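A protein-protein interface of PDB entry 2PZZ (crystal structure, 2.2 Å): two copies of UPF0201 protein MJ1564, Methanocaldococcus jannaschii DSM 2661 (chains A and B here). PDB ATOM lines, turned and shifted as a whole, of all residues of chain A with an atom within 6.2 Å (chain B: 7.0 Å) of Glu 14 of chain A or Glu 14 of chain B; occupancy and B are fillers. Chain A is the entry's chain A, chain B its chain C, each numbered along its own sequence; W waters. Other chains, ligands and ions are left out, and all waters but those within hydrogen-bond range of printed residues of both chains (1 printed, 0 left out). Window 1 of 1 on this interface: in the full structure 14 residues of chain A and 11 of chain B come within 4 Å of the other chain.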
ATOM      1  N   LYS A   9      -9.673   9.669  10.895  1.00  0.00           N
ATOM      2  CA  LYS A   9     -10.128  10.371   9.703  1.00  0.00           C
ATOM      3  C   LYS A   9     -10.421  11.816  10.097  1.00  0.00           C
ATOM      4  O   LYS A   9     -10.681  12.110  11.261  1.00  0.00           O
ATOM      5  CB  LYS A   9     -11.412   9.730   9.140  1.00  0.00           C
ATOM      6  CG  LYS A   9     -12.698  10.092   9.903  1.00  0.00           C
ATOM      7  CD  LYS A   9     -13.974   9.632   9.169  1.00  0.00           C
ATOM      8  CE  LYS A   9     -14.075   8.105   9.086  1.00  0.00           C
ATOM      9  NZ  LYS A   9     -15.410   7.613   8.586  1.00  0.00           N
ATOM     10  N   VAL A  10     -10.342  12.704   9.118  1.00  0.00           N
ATOM     11  CA  VAL A  10     -10.644  14.106   9.302  1.00  0.00           C
ATOM     12  C   VAL A  10     -11.692  14.382   8.239  1.00  0.00           C
ATOM     13  O   VAL A  10     -11.394  14.383   7.043  1.00  0.00           O
ATOM     14  CB  VAL A  10      -9.433  15.030   9.036  1.00  0.00           C
ATOM     15  CG1 VAL A  10      -9.903  16.499   9.029  1.00  0.00           C
ATOM     16  CG2 VAL A  10      -8.378  14.830  10.099  1.00  0.00           C
ATOM     17  N   LYS A  11     -12.925  14.590   8.673  1.00  0.00           N
ATOM     18  CA  LYS A  11     -14.000  14.865   7.731  1.00  0.00           C
ATOM     19  C   LYS A  11     -13.922  16.291   7.199  1.00  0.00           C
ATOM     20  O   LYS A  11     -13.315  17.168   7.825  1.00  0.00           O
ATOM     21  CB  LYS A  11     -15.335  14.600   8.412  1.00  0.00           C
ATOM     22  CG  LYS A  11     -15.484  13.139   8.832  1.00  0.00           C
ATOM     23  CD  LYS A  11     -16.922  12.839   9.231  1.00  0.00           C
ATOM     24  CE  LYS A  11     -17.138  11.353   9.388  1.00  0.00           C
ATOM     25  NZ  LYS A  11     -18.578  11.026   9.577  1.00  0.00           N
ATOM     26  N   PRO A  12     -14.523  16.540   6.019  1.00  0.00           N
ATOM     27  CA  PRO A  12     -14.527  17.863   5.384  1.00  0.00           C
ATOM     28  C   PRO A  12     -14.811  19.052   6.313  1.00  0.00           C
ATOM     29  O   PRO A  12     -14.181  20.102   6.181  1.00  0.00           O
ATOM     30  CB  PRO A  12     -15.599  17.715   4.303  1.00  0.00           C
ATOM     31  CG  PRO A  12     -15.377  16.293   3.839  1.00  0.00           C
ATOM     32  CD  PRO A  12     -15.222  15.550   5.170  1.00  0.00           C
ATOM     33  N   THR A  13     -15.759  18.895   7.241  1.00  0.00           N
ATOM     34  CA  THR A  13     -16.111  19.991   8.145  1.00  0.00           C
ATOM     35  C   THR A  13     -15.301  19.992   9.438  1.00  0.00           C
ATOM     36  O   THR A  13     -15.532  20.818  10.327  1.00  0.00           O
ATOM     37  CB  THR A  13     -17.622  19.973   8.513  1.00  0.00           C
ATOM     38  OG1 THR A  13     -17.946  18.754   9.191  1.00  0.00           O
ATOM     39  CG2 THR A  13     -18.475  20.109   7.258  1.00  0.00           C
ATOM     40  N   GLU A  14     -14.361  19.058   9.549  1.00  0.00           N
ATOM     41  CA  GLU A  14     -13.518  18.996  10.731  1.00  0.00           C
ATOM     42  C   GLU A  14     -12.262  19.817  10.489  1.00  0.00           C
ATOM     43  O   GLU A  14     -11.893  20.088   9.348  1.00  0.00           O
ATOM     44  CB  GLU A  14     -13.133  17.542  11.063  1.00  0.00           C
ATOM     45  CG  GLU A  14     -14.077  16.871  12.047  1.00  0.00           C
ATOM     46  CD  GLU A  14     -13.770  15.409  12.239  1.00  0.00           C
ATOM     47  OE1 GLU A  14     -13.561  14.979  13.401  1.00  0.00           O
ATOM     48  OE2 GLU A  14     -13.747  14.682  11.220  1.00  0.00           O
ATOM     49  N   ASP A  15     -11.627  20.241  11.575  1.00  0.00           N
ATOM     50  CA  ASP A  15     -10.380  20.995  11.474  1.00  0.00           C
ATOM     51  C   ASP A  15      -9.311  19.957  11.770  1.00  0.00           C
ATOM     52  O   ASP A  15      -9.236  19.443  12.886  1.00  0.00           O
ATOM     53  CB  ASP A  15     -10.328  22.099  12.524  1.00  0.00           C
ATOM     54  CG  ASP A  15      -9.015  22.851  12.507  1.00  0.00           C
ATOM     55  OD1 ASP A  15      -7.952  22.204  12.580  1.00  0.00           O
ATOM     56  OD2 ASP A  15      -9.045  24.094  12.424  1.00  0.00           O
ATOM     57  N   LYS A  16      -8.480  19.650  10.787  1.00  0.00           N
ATOM     58  CA  LYS A  16      -7.458  18.626  10.984  1.00  0.00           C
ATOM     59  C   LYS A  16      -6.565  18.834  12.203  1.00  0.00           C
ATOM     60  O   LYS A  16      -6.139  17.861  12.831  1.00  0.00           O
ATOM     61  CB  LYS A  16      -6.600  18.467   9.722  1.00  0.00           C
ATOM     62  CG  LYS A  16      -5.783  19.674   9.287  1.00  0.00           C
ATOM     63  CD  LYS A  16      -5.018  19.307   8.024  1.00  0.00           C
ATOM     64  CE  LYS A  16      -4.170  20.443   7.502  1.00  0.00           C
ATOM     65  NZ  LYS A  16      -3.404  20.032   6.284  1.00  0.00           N
ATOM     66  N   LYS A  18      -7.457  20.151  15.021  1.00  0.00           N
ATOM     67  CA  LYS A  18      -8.207  19.816  16.220  1.00  0.00           C
ATOM     68  C   LYS A  18      -8.234  18.302  16.379  1.00  0.00           C
ATOM     69  O   LYS A  18      -8.268  17.795  17.504  1.00  0.00           O
ATOM     70  CB  LYS A  18      -9.639  20.325  16.137  1.00  0.00           C
ATOM     71  CG  LYS A  18      -9.769  21.830  16.131  1.00  0.00           C
ATOM     72  CD  LYS A  18     -11.236  22.206  16.216  1.00  0.00           C
ATOM     73  CE  LYS A  18     -11.401  23.694  16.506  1.00  0.00           C
ATOM     74  NZ  LYS A  18     -12.845  24.068  16.607  1.00  0.00           N
ATOM     75  N   VAL A  19      -8.248  17.572  15.260  1.00  0.00           N
ATOM     76  CA  VAL A  19      -8.264  16.115  15.355  1.00  0.00           C
ATOM     77  C   VAL A  19      -6.888  15.700  15.833  1.00  0.00           C
ATOM     78  O   VAL A  19      -6.761  14.832  16.675  1.00  0.00           O
ATOM     79  CB  VAL A  19      -8.534  15.398  13.985  1.00  0.00           C
ATOM     80  CG1 VAL A  19      -8.386  13.867  14.168  1.00  0.00           C
ATOM     81  CG2 VAL A  19      -9.933  15.723  13.498  1.00  0.00           C
ATOM     82  N   LYS A  86     -13.521  10.763  19.547  1.00  0.00           N
ATOM     83  CA  LYS A  86     -12.737  11.901  19.099  1.00  0.00           C
ATOM     84  C   LYS A  86     -13.079  13.193  19.844  1.00  0.00           C
ATOM     85  O   LYS A  86     -12.199  14.032  20.077  1.00  0.00           O
ATOM     86  CB  LYS A  86     -12.947  12.066  17.585  1.00  0.00           C
ATOM     87  CG  LYS A  86     -11.839  12.766  16.851  1.00  0.00           C
ATOM     88  CD  LYS A  86     -11.672  12.225  15.422  1.00  0.00           C
ATOM     89  CE  LYS A  86     -12.968  12.243  14.638  1.00  0.00           C
ATOM     90  NZ  LYS A  86     -12.739  12.206  13.159  1.00  0.00           N
ATOM     91  N   GLN A  87     -14.348  13.339  20.232  1.00  0.00           N
ATOM     92  CA  GLN A  87     -14.809  14.545  20.923  1.00  0.00           C
ATOM     93  C   GLN A  87     -14.391  14.524  22.386  1.00  0.00           C
ATOM     94  O   GLN A  87     -13.995  15.549  22.947  1.00  0.00           O
ATOM     95  CB  GLN A  87     -16.333  14.666  20.784  1.00  0.00           C
ATOM     96  CG  GLN A  87     -16.816  14.422  19.343  1.00  0.00           C
ATOM     97  CD  GLN A  87     -16.068  15.278  18.332  1.00  0.00           C
ATOM     98  OE1 GLN A  87     -15.884  14.885  17.171  1.00  0.00           O
ATOM     99  NE2 GLN A  87     -15.635  16.459  18.760  1.00  0.00           N
ATOM    100  N   ASP A  99     -17.406   8.253  18.073  1.00  0.00           N
ATOM    101  CA  ASP A  99     -18.237   9.442  17.917  1.00  0.00           C
ATOM    102  C   ASP A  99     -18.785   9.501  16.493  1.00  0.00           C
ATOM    103  O   ASP A  99     -18.398   8.702  15.631  1.00  0.00           O
ATOM    104  CB  ASP A  99     -17.436  10.715  18.211  1.00  0.00           C
ATOM    105  CG  ASP A  99     -16.248  10.881  17.289  1.00  0.00           C
ATOM    106  OD1 ASP A  99     -15.271  10.114  17.438  1.00  0.00           O
ATOM    107  OD2 ASP A  99     -16.296  11.776  16.414  1.00  0.00           O
ATOM    108  N   HIS A 101     -18.070  11.289  14.233  1.00  0.00           N
ATOM    109  CA  HIS A 101     -17.022  11.542  13.255  1.00  0.00           C
ATOM    110  C   HIS A 101     -15.942  10.474  13.053  1.00  0.00           C
ATOM    111  O   HIS A 101     -14.905  10.753  12.463  1.00  0.00           O
ATOM    112  CB  HIS A 101     -16.396  12.914  13.531  1.00  0.00           C
ATOM    113  CG  HIS A 101     -17.305  14.056  13.196  1.00  0.00           C
ATOM    114  ND1 HIS A 101     -18.623  14.097  13.593  1.00  0.00           N
ATOM    115  CD2 HIS A 101     -17.093  15.188  12.487  1.00  0.00           C
ATOM    116  CE1 HIS A 101     -19.187  15.203  13.141  1.00  0.00           C
ATOM    117  NE2 HIS A 101     -18.279  15.883  12.467  1.00  0.00           N
ATOM    118  N   ALA B   8     -27.964  22.635  12.553  1.00  0.00           N
ATOM    119  CA  ALA B   8     -26.785  21.789  12.395  1.00  0.00           C
ATOM    120  C   ALA B   8     -25.948  21.869  13.665  1.00  0.00           C
ATOM    121  O   ALA B   8     -25.745  22.956  14.216  1.00  0.00           O
ATOM    122  CB  ALA B   8     -25.965  22.243  11.216  1.00  0.00           C
ATOM    123  N   LYS B   9     -25.480  20.718  14.133  1.00  0.00           N
ATOM    124  CA  LYS B   9     -24.648  20.670  15.319  1.00  0.00           C
ATOM    125  C   LYS B   9     -23.182  20.841  14.912  1.00  0.00           C
ATOM    126  O   LYS B   9     -22.808  20.555  13.777  1.00  0.00           O
ATOM    127  CB  LYS B   9     -24.848  19.333  16.047  1.00  0.00           C
ATOM    128  CG  LYS B   9     -26.302  19.073  16.444  1.00  0.00           C
ATOM    129  CD  LYS B   9     -26.512  17.670  16.987  1.00  0.00           C
ATOM    130  CE  LYS B   9     -27.990  17.397  17.268  1.00  0.00           C
ATOM    131  NZ  LYS B   9     -28.236  15.975  17.680  1.00  0.00           N
ATOM    132  N   VAL B  10     -22.370  21.345  15.837  1.00  0.00           N
ATOM    133  CA  VAL B  10     -20.942  21.530  15.607  1.00  0.00           C
ATOM    134  C   VAL B  10     -20.213  20.858  16.774  1.00  0.00           C
ATOM    135  O   VAL B  10     -20.304  21.304  17.927  1.00  0.00           O
ATOM    136  CB  VAL B  10     -20.546  23.022  15.566  1.00  0.00           C
ATOM    137  CG1 VAL B  10     -19.035  23.152  15.372  1.00  0.00           C
ATOM    138  CG2 VAL B  10     -21.274  23.726  14.440  1.00  0.00           C
ATOM    139  N   LYS B  11     -19.507  19.771  16.470  1.00  0.00           N
ATOM    140  CA  LYS B  11     -18.782  19.027  17.485  1.00  0.00           C
ATOM    141  C   LYS B  11     -17.458  19.717  17.811  1.00  0.00           C
ATOM    142  O   LYS B  11     -17.011  20.611  17.091  1.00  0.00           O
ATOM    143  CB  LYS B  11     -18.491  17.609  16.983  1.00  0.00           C
ATOM    144  CG  LYS B  11     -19.707  16.855  16.437  1.00  0.00           C
ATOM    145  CD  LYS B  11     -20.692  16.502  17.534  1.00  0.00           C
ATOM    146  CE  LYS B  11     -21.871  15.710  16.974  1.00  0.00           C
ATOM    147  NZ  LYS B  11     -22.886  15.385  18.022  1.00  0.00           N
ATOM    148  N   PRO B  12     -16.816  19.315  18.911  1.00  0.00           N
ATOM    149  CA  PRO B  12     -15.537  19.913  19.292  1.00  0.00           C
ATOM    150  C   PRO B  12     -14.492  19.916  18.172  1.00  0.00           C
ATOM    151  O   PRO B  12     -13.818  20.921  17.963  1.00  0.00           O
ATOM    152  CB  PRO B  12     -15.118  19.062  20.483  1.00  0.00           C
ATOM    153  CG  PRO B  12     -16.436  18.861  21.171  1.00  0.00           C
ATOM    154  CD  PRO B  12     -17.356  18.496  20.014  1.00  0.00           C
ATOM    155  N   THR B  13     -14.371  18.810  17.435  1.00  0.00           N
ATOM    156  CA  THR B  13     -13.369  18.732  16.369  1.00  0.00           C
ATOM    157  C   THR B  13     -13.758  19.409  15.065  1.00  0.00           C
ATOM    158  O   THR B  13     -12.956  19.427  14.129  1.00  0.00           O
ATOM    159  CB  THR B  13     -12.971  17.256  16.043  1.00  0.00           C
ATOM    160  OG1 THR B  13     -14.116  16.525  15.580  1.00  0.00           O
ATOM    161  CG2 THR B  13     -12.427  16.572  17.274  1.00  0.00           C
ATOM    162  N   GLU B  14     -14.971  19.967  14.998  1.00  0.00           N
ATOM    163  CA  GLU B  14     -15.416  20.652  13.780  1.00  0.00           C
ATOM    164  C   GLU B  14     -15.075  22.146  13.744  1.00  0.00           C
ATOM    165  O   GLU B  14     -14.809  22.772  14.775  1.00  0.00           O
ATOM    166  CB  GLU B  14     -16.938  20.504  13.580  1.00  0.00           C
ATOM    167  CG  GLU B  14     -17.405  19.076  13.302  1.00  0.00           C
ATOM    168  CD  GLU B  14     -18.849  19.004  12.835  1.00  0.00           C
ATOM    169  OE1 GLU B  14     -19.096  19.193  11.624  1.00  0.00           O
ATOM    170  OE2 GLU B  14     -19.742  18.763  13.678  1.00  0.00           O
ATOM    171  N   ASP B  15     -15.093  22.694  12.533  1.00  0.00           N
ATOM    172  CA  ASP B  15     -14.845  24.111  12.275  1.00  0.00           C
ATOM    173  C   ASP B  15     -16.249  24.690  12.071  1.00  0.00           C
ATOM    174  O   ASP B  15     -16.884  24.411  11.056  1.00  0.00           O
ATOM    175  CB  ASP B  15     -14.026  24.274  10.991  1.00  0.00           C
ATOM    176  CG  ASP B  15     -13.724  25.730  10.663  1.00  0.00           C
ATOM    177  OD1 ASP B  15     -14.618  26.581  10.835  1.00  0.00           O
ATOM    178  OD2 ASP B  15     -12.599  26.023  10.214  1.00  0.00           O
ATOM    179  N   LYS B  16     -16.728  25.495  13.020  1.00  0.00           N
ATOM    180  CA  LYS B  16     -18.078  26.044  12.928  1.00  0.00           C
ATOM    181  C   LYS B  16     -18.378  26.691  11.593  1.00  0.00           C
ATOM    182  O   LYS B  16     -19.510  26.613  11.099  1.00  0.00           O
ATOM    183  CB  LYS B  16     -18.353  27.026  14.079  1.00  0.00           C
ATOM    184  CG  LYS B  16     -17.481  28.287  14.136  1.00  0.00           C
ATOM    185  CD  LYS B  16     -17.682  29.046  15.469  1.00  0.00           C
ATOM    186  CE  LYS B  16     -16.715  30.227  15.603  1.00  0.00           C
ATOM    187  NZ  LYS B  16     -16.782  30.944  16.931  1.00  0.00           N
ATOM    188  N   TYR B  17     -17.348  27.289  10.993  1.00  0.00           N
ATOM    189  CA  TYR B  17     -17.492  27.969   9.727  1.00  0.00           C
ATOM    190  C   TYR B  17     -17.513  27.071   8.501  1.00  0.00           C
ATOM    191  O   TYR B  17     -18.017  27.475   7.452  1.00  0.00           O
ATOM    192  CB  TYR B  17     -16.422  29.050   9.599  1.00  0.00           C
ATOM    193  CG  TYR B  17     -16.793  30.260  10.422  1.00  0.00           C
ATOM    194  CD1 TYR B  17     -17.778  31.153   9.980  1.00  0.00           C
ATOM    195  CD2 TYR B  17     -16.251  30.451  11.685  1.00  0.00           C
ATOM    196  CE1 TYR B  17     -18.217  32.201  10.791  1.00  0.00           C
ATOM    197  CE2 TYR B  17     -16.679  31.492  12.505  1.00  0.00           C
ATOM    198  CZ  TYR B  17     -17.662  32.357  12.057  1.00  0.00           C
ATOM    199  OH  TYR B  17     -18.109  33.342  12.895  1.00  0.00           O
ATOM    200  N   LYS B  18     -16.969  25.862   8.630  1.00  0.00           N
ATOM    201  CA  LYS B  18     -17.004  24.912   7.521  1.00  0.00           C
ATOM    202  C   LYS B  18     -18.423  24.364   7.554  1.00  0.00           C
ATOM    203  O   LYS B  18     -19.021  24.096   6.516  1.00  0.00           O
ATOM    204  CB  LYS B  18     -15.986  23.782   7.724  1.00  0.00           C
ATOM    205  CG  LYS B  18     -14.539  24.237   7.541  1.00  0.00           C
ATOM    206  CD  LYS B  18     -13.550  23.069   7.682  1.00  0.00           C
ATOM    207  CE  LYS B  18     -12.163  23.473   7.197  1.00  0.00           C
ATOM    208  NZ  LYS B  18     -11.170  22.368   7.395  1.00  0.00           N
ATOM    209  N   VAL B  19     -18.964  24.210   8.760  1.00  0.00           N
ATOM    210  CA  VAL B  19     -20.334  23.728   8.910  1.00  0.00           C
ATOM    211  C   VAL B  19     -21.263  24.781   8.316  1.00  0.00           C
ATOM    212  O   VAL B  19     -22.179  24.459   7.556  1.00  0.00           O
ATOM    213  CB  VAL B  19     -20.705  23.507  10.400  1.00  0.00           C
ATOM    214  CG1 VAL B  19     -22.190  23.183  10.535  1.00  0.00           C
ATOM    215  CG2 VAL B  19     -19.881  22.362  10.978  1.00  0.00           C
ATOM    216  N   GLU B  40     -17.098  22.380  24.408  1.00  0.00           N
ATOM    217  CA  GLU B  40     -16.749  22.704  23.029  1.00  0.00           C
ATOM    218  C   GLU B  40     -17.795  22.368  21.952  1.00  0.00           C
ATOM    219  O   GLU B  40     -17.498  22.416  20.760  1.00  0.00           O
ATOM    220  CB  GLU B  40     -15.410  22.052  22.665  1.00  0.00           C
ATOM    221  CG  GLU B  40     -14.227  22.478  23.549  1.00  0.00           C
ATOM    222  CD  GLU B  40     -13.846  23.944  23.380  1.00  0.00           C
ATOM    223  OE1 GLU B  40     -13.406  24.337  22.272  1.00  0.00           O
ATOM    224  OE2 GLU B  40     -13.990  24.703  24.362  1.00  0.00           O
ATOM    225  N   GLY B  42     -21.404  23.051  19.835  1.00  0.00           N
ATOM    226  CA  GLY B  42     -22.081  24.246  19.354  1.00  0.00           C
ATOM    227  C   GLY B  42     -23.159  23.885  18.341  1.00  0.00           C
ATOM    228  O   GLY B  42     -23.293  22.724  17.973  1.00  0.00           O
ATOM    229  N   LYS B  86     -23.947  16.498   5.918  1.00  0.00           N
ATOM    230  CA  LYS B  86     -23.074  17.670   6.061  1.00  0.00           C
ATOM    231  C   LYS B  86     -21.851  17.651   5.173  1.00  0.00           C
ATOM    232  O   LYS B  86     -21.535  18.644   4.502  1.00  0.00           O
ATOM    233  CB  LYS B  86     -22.599  17.809   7.516  1.00  0.00           C
ATOM    234  CG  LYS B  86     -23.653  18.315   8.459  1.00  0.00           C
ATOM    235  CD  LYS B  86     -23.265  18.080   9.923  1.00  0.00           C
ATOM    236  CE  LYS B  86     -22.029  18.872  10.344  1.00  0.00           C
ATOM    237  NZ  LYS B  86     -21.788  18.621  11.800  1.00  0.00           N
ATOM    238  N   GLN B  87     -21.147  16.527   5.178  1.00  0.00           N
ATOM    239  CA  GLN B  87     -19.926  16.412   4.386  1.00  0.00           C
ATOM    240  C   GLN B  87     -20.185  16.574   2.885  1.00  0.00           C
ATOM    241  O   GLN B  87     -19.389  17.187   2.174  1.00  0.00           O
ATOM    242  CB  GLN B  87     -19.238  15.081   4.710  1.00  0.00           C
ATOM    243  CG  GLN B  87     -19.133  14.828   6.213  1.00  0.00           C
ATOM    244  CD  GLN B  87     -18.460  15.993   6.988  1.00  0.00           C
ATOM    245  OE1 GLN B  87     -18.668  16.146   8.193  1.00  0.00           O
ATOM    246  NE2 GLN B  87     -17.663  16.792   6.301  1.00  0.00           N
HETATM  247  O   HOH W   1     -11.478  25.353  13.399  1.00  0.00           O
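The side-chain carboxylate (OE1) of Glu 14 of chain B sits at hydrogen-bond distance from the side-chain hydroxyl (OG1) of Thr 13 of chain A (2.7 Å). The backbone NH (N) of Asp 15 of chain B lies within hydrogen-bond range of the backbone carbonyl oxygen (O) of Thr 13 of chain A, 2.9 Å away. The side-chain hydroxyl (OG1) of Thr 13 of chain A lies within hydrogen-bond range of the side-chain amide oxygen (OE1) of Gln 87 of chain B (2.9 Å). The side-chain carboxylate (OE1) of Glu 14 of chain A sits at hydrogen-bond distance from the side-chain hydroxyl (OG1) of Thr 13 of chain B, 2.7 Å away. The side-chain amino group (NZ) of Lys 18 of chain B lies within hydrogen-bond range of the backbone carbonyl oxygen (O) of Glu 14 of chain A. The backbone carbonyl oxygen (O) of Thr 13 of chain B lies within hydrogen-bond range of the backbone NH (N) of Asp 15 of chain A (3.0 Å). NZ of Lys 18 of chain A lies within hydrogen-bond range of O of Glu 14 of chain B, at 3.0 Å. The side-chain amide oxygen (OE1) of Gln 87 of chain A is in hydrogen-bond range of the side-chain hydroxyl (OG1) of Thr 13 of chain B (2.9 Å). A ring nitrogen (NE2) of His 101 of chain A lies close to the side-chain carboxylate (OE2) of Glu 14 of chain B (3.4 Å). The backbone nitrogen of Pro 12 of chain A sits close to the side-chain amide nitrogen of Gln 87 of chain B (3.2 Å). The side-chain amide nitrogen (NE2) of Gln 87 of chain A sits close to the backbone nitrogen (N) of Pro 12 of chain B (3.1 Å).
The side-chain amino group (NZ) of Lys 86 of chain A is in hydrogen-bond range of the backbone carbonyl oxygen (O) of Lys 9 of chain A. The backbone NH (N) of Lys 11 of chain A lies within hydrogen-bond range of the side-chain carboxylate (OE2) of Glu 14 of chain A. The side-chain carboxylate (OE1) of Glu 14 of chain A lies within salt-bridge range of the side-chain amino group (NZ) of Lys 86 of chain A, 2.9 Å away. The side-chain amino group of Lys 86 of chain A is in hydrogen-bond range of the backbone carbonyl oxygen of His 101 of chain A (2.7 Å). NZ of Lys 86 of chain B lies within salt-bridge range of OE1 of Glu 14 of chain B (2.8 Å). OD1 of Asp 15 of chain B sits at hydrogen-bond distance from N of Tyr 17 of chain B (2.8 Å).
Gln 87 of chain B touches Lys 11 of chain A (OE1 to CB, 3.7 Å). CD of Lys 18 of chain B touches O of Pro 12 of chain A, 3.4 Å away. Lys 18 of chain B touches Thr 13 of chain A (CB to CA, 3.8 Å). CA of Glu 14 of chain B touches CA of Glu 14 of chain A, 3.95 Å away. Pro 12 of chain B touches Lys 18 of chain A. O of Thr 13 of chain B touches CD of Lys 18 of chain A (3.9 Å). Thr 13 of chain B touches Lys 86 of chain A (CG2 to O, 3.8 Å). Lys 11 of chain B touches Gln 87 of chain A. His 101 of chain A touches Lys 11 of chain B (CE1 to CG, 3.7 Å).
Val 10 of chain A touches none of the printed residues of chain B. Of the printed residues of chain B, Lys 11 of chain A touches Gln 87. Glu 14 of chain A touches just these residues of chain B: Thr 13 (2.7 Å), Glu 14 (3.95 Å) and Lys 18 (3.1 Å). Printed residues of chain B within 4 Å of Gln 87 of chain A: Lys 11 (3.6 Å), Pro 12 (2.9 Å) and Thr 13 (2.9 Å). Printed residues of chain A within 4 Å of Pro 12 of chain B: Lys 18 and Gln 87. Of chain A, only Thr 13 (2.7 Å), Glu 14 (3.95 Å), Lys 18 (3.0 Å) and His 101 (3.2 Å) come within 4 Å of Glu 14 of chain B. Gly 42 of chain B touches none of the printed residues of chain A. The nearest residue of chain A that does not touch Glu 14 of chain B is Asp 15 of chain A (4.4 Å).
Of the 14 printed residues of chain A, 9 touch a printed residue of chain B.
Pro 12 of chain A touches Lys 18 of chain B, and with the chains exchanged Lys 18 of chain A touches Pro 12 of chain B. Thr 13 of chain A touches Lys 18 of chain B, and with the chains exchanged Lys 18 of chain A touches Thr 13 of chain B. Glu 14 of chain A touches Lys 18 of chain B, and with the chains exchanged Lys 18 of chain A touches Glu 14 of chain B. Lys 86 of chain A touches Thr 13 of chain B, but with the chains exchanged Thr 13 of chain A does not touch Lys 86 of chain B (4.2 Å). Positions printed for both chains: 9, 10, 11, 12, 13, 14, 15, 16, 18, 19, 86 and 87.
Water W1 lies within hydrogen-bond range of OD2 of Asp 15 of chain A (2.9 Å) and OD2 of Asp 15 of chain B (3.4 Å).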
